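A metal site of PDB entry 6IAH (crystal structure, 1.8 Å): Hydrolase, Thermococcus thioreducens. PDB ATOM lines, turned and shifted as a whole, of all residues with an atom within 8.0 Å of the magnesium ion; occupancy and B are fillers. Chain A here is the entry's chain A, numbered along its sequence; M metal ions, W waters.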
ATOM      1  N   PHE A   5      10.412 -21.537  21.730  1.00  0.00           N
ATOM      2  CA  PHE A   5      10.304 -22.935  22.206  1.00  0.00           C
ATOM      3  C   PHE A   5       8.855 -23.250  22.636  1.00  0.00           C
ATOM      4  O   PHE A   5       8.109 -22.417  23.197  1.00  0.00           O
ATOM      5  CB  PHE A   5      11.165 -23.183  23.455  1.00  0.00           C
ATOM      6  CG  PHE A   5      12.563 -22.687  23.367  1.00  0.00           C
ATOM      7  CD1 PHE A   5      13.552 -23.497  22.837  1.00  0.00           C
ATOM      8  CD2 PHE A   5      12.913 -21.417  23.910  1.00  0.00           C
ATOM      9  CE1 PHE A   5      14.851 -23.051  22.776  1.00  0.00           C
ATOM     10  CE2 PHE A   5      14.208 -20.969  23.859  1.00  0.00           C
ATOM     11  CZ  PHE A   5      15.201 -21.805  23.301  1.00  0.00           C
ATOM     12  N   ASP A   6       8.462 -24.486  22.370  1.00  0.00           N
ATOM     13  CA  ASP A   6       7.463 -25.183  23.178  1.00  0.00           C
ATOM     14  C   ASP A   6       8.126 -25.512  24.523  1.00  0.00           C
ATOM     15  O   ASP A   6       9.360 -25.551  24.628  1.00  0.00           O
ATOM     16  CB  ASP A   6       7.057 -26.484  22.442  1.00  0.00           C
ATOM     17  CG  ASP A   6       5.962 -27.302  23.182  1.00  0.00           C
ATOM     18  OD1 ASP A   6       5.018 -26.732  23.766  1.00  0.00           O
ATOM     19  OD2 ASP A   6       6.085 -28.544  23.162  1.00  0.00           O
ATOM     20  N   VAL A   7       7.319 -25.752  25.556  1.00  0.00           N
ATOM     21  CA  VAL A   7       7.842 -26.144  26.854  1.00  0.00           C
ATOM     22  C   VAL A   7       7.804 -27.660  26.966  1.00  0.00           C
ATOM     23  O   VAL A   7       8.845 -28.281  27.062  1.00  0.00           O
ATOM     24  CB  VAL A   7       7.083 -25.464  27.978  1.00  0.00           C
ATOM     25  CG1 VAL A   7       7.559 -25.907  29.342  1.00  0.00           C
ATOM     26  CG2 VAL A   7       7.227 -23.976  27.861  1.00  0.00           C
ATOM     27  N   ASP A   8       6.623 -28.241  26.943  1.00  0.00           N
ATOM     28  CA  ASP A   8       6.475 -29.691  27.308  1.00  0.00           C
ATOM     29  C   ASP A   8       6.977 -30.600  26.184  1.00  0.00           C
ATOM     30  O   ASP A   8       6.475 -30.531  25.080  1.00  0.00           O
ATOM     31  CB  ASP A   8       4.995 -30.015  27.624  1.00  0.00           C
ATOM     32  CG  ASP A   8       4.464 -29.319  28.923  1.00  0.00           C
ATOM     33  OD1 ASP A   8       5.210 -28.627  29.661  1.00  0.00           O
ATOM     34  OD2 ASP A   8       3.264 -29.493  29.234  1.00  0.00           O
ATOM     35  N   GLY A   9       7.939 -31.464  26.475  1.00  0.00           N
ATOM     36  CA  GLY A   9       8.552 -32.346  25.510  1.00  0.00           C
ATOM     37  C   GLY A   9       9.777 -31.695  24.831  1.00  0.00           C
ATOM     38  O   GLY A   9      10.434 -32.384  24.045  1.00  0.00           O
ATOM     39  N   VAL A  10      10.036 -30.390  25.078  1.00  0.00           N
ATOM     40  CA  VAL A  10      11.174 -29.678  24.491  1.00  0.00           C
ATOM     41  C   VAL A  10      12.084 -29.165  25.609  1.00  0.00           C
ATOM     42  O   VAL A  10      13.241 -29.609  25.719  1.00  0.00           O
ATOM     43  CB  VAL A  10      10.701 -28.504  23.587  1.00  0.00           C
ATOM     44  CG1 VAL A  10      11.869 -27.639  23.159  1.00  0.00           C
ATOM     45  CG2 VAL A  10       9.954 -29.031  22.363  1.00  0.00           C
ATOM     46  N   LEU A  11      11.628 -28.183  26.411  1.00  0.00           N
ATOM     47  CA  LEU A  11      12.419 -27.711  27.570  1.00  0.00           C
ATOM     48  C   LEU A  11      12.293 -28.609  28.791  1.00  0.00           C
ATOM     49  O   LEU A  11      13.230 -28.656  29.586  1.00  0.00           O
ATOM     50  CB  LEU A  11      12.034 -26.291  27.960  1.00  0.00           C
ATOM     51  CG  LEU A  11      12.128 -25.296  26.791  1.00  0.00           C
ATOM     52  CD1 LEU A  11      11.629 -23.893  27.179  1.00  0.00           C
ATOM     53  CD2 LEU A  11      13.529 -25.190  26.213  1.00  0.00           C
ATOM     54  N   ILE A  12      11.107 -29.200  28.990  1.00  0.00           N
ATOM     55  CA  ILE A  12      10.763 -29.974  30.201  1.00  0.00           C
ATOM     56  C   ILE A  12      10.208 -31.330  29.794  1.00  0.00           C
ATOM     57  O   ILE A  12       9.329 -31.425  28.898  1.00  0.00           O
ATOM     58  CB  ILE A  12       9.705 -29.231  31.056  1.00  0.00           C
ATOM     59  CG1 ILE A  12      10.353 -27.971  31.662  1.00  0.00           C
ATOM     60  CG2 ILE A  12       9.215 -30.106  32.202  1.00  0.00           C
ATOM     61  CD1 ILE A  12       9.381 -27.041  32.351  1.00  0.00           C
ATOM     62  N   VAL A  14       7.829 -33.883  30.938  1.00  0.00           N
ATOM     63  CA  VAL A  14       6.701 -33.895  31.874  1.00  0.00           C
ATOM     64  C   VAL A  14       6.410 -35.316  32.138  1.00  0.00           C
ATOM     65  O   VAL A  14       5.211 -35.698  32.084  1.00  0.00           O
ATOM     66  CB  VAL A  14       5.457 -33.137  31.392  1.00  0.00           C
ATOM     67  CG1 VAL A  14       5.824 -31.653  31.250  1.00  0.00           C
ATOM     68  CG2 VAL A  14       4.869 -33.676  30.072  1.00  0.00           C
ATOM     69  N   VAL A 149       6.010 -20.324  23.296  1.00  0.00           N
ATOM     70  CA  VAL A 149       4.552 -20.371  23.078  1.00  0.00           C
ATOM     71  C   VAL A 149       4.159 -21.655  23.684  1.00  0.00           C
ATOM     72  O   VAL A 149       4.637 -22.700  23.223  1.00  0.00           O
ATOM     73  CB  VAL A 149       4.162 -20.312  21.578  1.00  0.00           C
ATOM     74  CG1 VAL A 149       2.677 -20.484  21.399  1.00  0.00           C
ATOM     75  CG2 VAL A 149       4.664 -19.023  20.922  1.00  0.00           C
ATOM     76  N   THR A 150       3.248 -21.629  24.651  1.00  0.00           N
ATOM     77  CA  THR A 150       2.940 -22.863  25.403  1.00  0.00           C
ATOM     78  C   THR A 150       1.461 -22.935  25.720  1.00  0.00           C
ATOM     79  O   THR A 150       0.814 -21.936  25.943  1.00  0.00           O
ATOM     80  CB  THR A 150       3.830 -22.965  26.664  1.00  0.00           C
ATOM     81  OG1 THR A 150       3.597 -24.175  27.395  1.00  0.00           O
ATOM     82  CG2 THR A 150       3.655 -21.823  27.566  1.00  0.00           C
ATOM     83  N   GLY A 151       0.933 -24.154  25.811  1.00  0.00           N
ATOM     84  CA  GLY A 151      -0.414 -24.385  26.326  1.00  0.00           C
ATOM     85  C   GLY A 151      -0.519 -24.204  27.842  1.00  0.00           C
ATOM     86  O   GLY A 151      -1.632 -24.186  28.379  1.00  0.00           O
ATOM     87  N   LYS A 179      -1.934 -22.779  20.315  1.00  0.00           N
ATOM     88  CA  LYS A 179      -1.487 -23.456  19.104  1.00  0.00           C
ATOM     89  C   LYS A 179      -2.658 -24.353  18.638  1.00  0.00           C
ATOM     90  O   LYS A 179      -3.343 -24.905  19.483  1.00  0.00           O
ATOM     91  CB  LYS A 179      -0.263 -24.363  19.387  1.00  0.00           C
ATOM     92  CG  LYS A 179       0.961 -23.530  19.730  1.00  0.00           C
ATOM     93  CD  LYS A 179       2.186 -24.353  19.961  1.00  0.00           C
ATOM     94  CE  LYS A 179       2.128 -25.021  21.312  1.00  0.00           C
ATOM     95  NZ  LYS A 179       3.307 -25.847  21.635  1.00  0.00           N
ATOM     96  N   TYR A 196      10.892 -22.024  15.473  1.00  0.00           N
ATOM     97  CA  TYR A 196      10.123 -22.590  16.558  1.00  0.00           C
ATOM     98  C   TYR A 196      10.607 -24.008  16.747  1.00  0.00           C
ATOM     99  O   TYR A 196      10.675 -24.736  15.793  1.00  0.00           O
ATOM    100  CB  TYR A 196       8.625 -22.610  16.262  1.00  0.00           C
ATOM    101  CG  TYR A 196       7.779 -22.960  17.475  1.00  0.00           C
ATOM    102  CD1 TYR A 196       7.577 -22.039  18.511  1.00  0.00           C
ATOM    103  CD2 TYR A 196       7.213 -24.227  17.634  1.00  0.00           C
ATOM    104  CE1 TYR A 196       6.837 -22.380  19.641  1.00  0.00           C
ATOM    105  CE2 TYR A 196       6.446 -24.568  18.744  1.00  0.00           C
ATOM    106  CZ  TYR A 196       6.264 -23.657  19.757  1.00  0.00           C
ATOM    107  OH  TYR A 196       5.541 -24.015  20.883  1.00  0.00           O
ATOM    108  N   ILE A 197      10.865 -24.378  18.002  1.00  0.00           N
ATOM    109  CA  ILE A 197      11.296 -25.768  18.393  1.00  0.00           C
ATOM    110  C   ILE A 197      10.137 -26.474  19.088  1.00  0.00           C
ATOM    111  O   ILE A 197       9.741 -26.030  20.165  1.00  0.00           O
ATOM    112  CB  ILE A 197      12.482 -25.721  19.359  1.00  0.00           C
ATOM    113  CG1 ILE A 197      13.546 -24.676  18.961  1.00  0.00           C
ATOM    114  CG2 ILE A 197      13.060 -27.135  19.556  1.00  0.00           C
ATOM    115  CD1 ILE A 197      14.013 -24.750  17.544  1.00  0.00           C
ATOM    116  N   GLY A 198       9.594 -27.547  18.450  1.00  0.00           N
ATOM    117  CA  GLY A 198       8.453 -28.301  18.935  1.00  0.00           C
ATOM    118  C   GLY A 198       8.851 -29.772  19.062  1.00  0.00           C
ATOM    119  O   GLY A 198       9.943 -30.135  18.657  1.00  0.00           O
ATOM    120  N   ASP A 199       7.987 -30.536  19.688  1.00  0.00           N
ATOM    121  CA  ASP A 199       8.100 -32.022  19.769  1.00  0.00           C
ATOM    122  C   ASP A 199       6.924 -32.756  19.070  1.00  0.00           C
ATOM    123  O   ASP A 199       6.971 -33.924  18.934  1.00  0.00           O
ATOM    124  CB  ASP A 199       8.240 -32.433  21.224  1.00  0.00           C
ATOM    125  CG  ASP A 199       6.989 -32.190  22.059  1.00  0.00           C
ATOM    126  OD1 ASP A 199       6.447 -31.039  22.128  1.00  0.00           O
ATOM    127  OD2 ASP A 199       6.524 -33.149  22.697  1.00  0.00           O
ATOM    128  N   THR A 200       5.871 -32.069  18.635  1.00  0.00           N
ATOM    129  CA  THR A 200       4.709 -32.771  18.085  1.00  0.00           C
ATOM    130  C   THR A 200       4.310 -32.267  16.727  1.00  0.00           C
ATOM    131  O   THR A 200       4.704 -31.191  16.338  1.00  0.00           O
ATOM    132  CB  THR A 200       3.461 -32.689  19.003  1.00  0.00           C
ATOM    133  OG1 THR A 200       2.996 -31.330  19.081  1.00  0.00           O
ATOM    134  CG2 THR A 200       3.735 -33.283  20.323  1.00  0.00           C
ATOM    135  N   ASP A 203       2.697 -28.800  16.724  1.00  0.00           N
ATOM    136  CA  ASP A 203       3.715 -27.746  16.637  1.00  0.00           C
ATOM    137  C   ASP A 203       4.114 -27.446  15.185  1.00  0.00           C
ATOM    138  O   ASP A 203       4.261 -26.278  14.770  1.00  0.00           O
ATOM    139  CB  ASP A 203       4.952 -28.103  17.458  1.00  0.00           C
ATOM    140  CG  ASP A 203       4.660 -28.190  18.960  1.00  0.00           C
ATOM    141  OD1 ASP A 203       3.891 -27.343  19.512  1.00  0.00           O
ATOM    142  OD2 ASP A 203       5.181 -29.146  19.578  1.00  0.00           O
ATOM    143  N   VAL A 222      12.241 -31.760  17.771  1.00  0.00           N
ATOM    144  CA  VAL A 222      13.172 -32.528  18.578  1.00  0.00           C
ATOM    145  C   VAL A 222      12.921 -33.997  18.396  1.00  0.00           C
ATOM    146  O   VAL A 222      11.764 -34.389  18.242  1.00  0.00           O
ATOM    147  CB  VAL A 222      13.212 -32.102  20.047  1.00  0.00           C
ATOM    148  CG1 VAL A 222      13.659 -30.650  20.123  1.00  0.00           C
ATOM    149  CG2 VAL A 222      11.869 -32.328  20.742  1.00  0.00           C
HETATM  150 MG    MG M   1       5.145 -30.191  23.441  1.00  0.00          MG
HETATM  151  O   HOH W   1       4.019 -29.910  21.673  1.00  0.00           O
HETATM  152  O   HOH W   2       4.503 -32.009  23.918  1.00  0.00           O
HETATM  153  O   HOH W   3       3.722 -29.336  24.558  1.00  0.00           O
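The nearest printed residue that does not touch the magnesium ion is Asp 203 (4.002 Å).
The backbone NH of Asp 199 lies within hydrogen-bond range of the side-chain carboxylate of Asp 203 (3.1 Å).
N of Asp 6 lies close to OH of Tyr 196 (3.3 Å).
N of Asp 6 is in hydrogen-bond range of O of Ile 197 (3.0 Å).
NZ of Lys 179 is in salt-bridge range of OD1 of Asp 6, 2.9 Å away.
Water W1 lies within hydrogen-bond range of OD2 of Asp 203 and OG1 of Thr 200.
The magnesium ion is bound by the side-chain carboxylate of Asp 6 (1.9 Å), water W2 (2.0 Å), water W3 (2.0 Å), the side-chain carboxylate of Asp 199 (2.0 Å), water W1 (2.1 Å) and the backbone carbonyl oxygen of Asp 8 (2.1 Å).
The magnesium ion has six donor atoms within binding distance.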
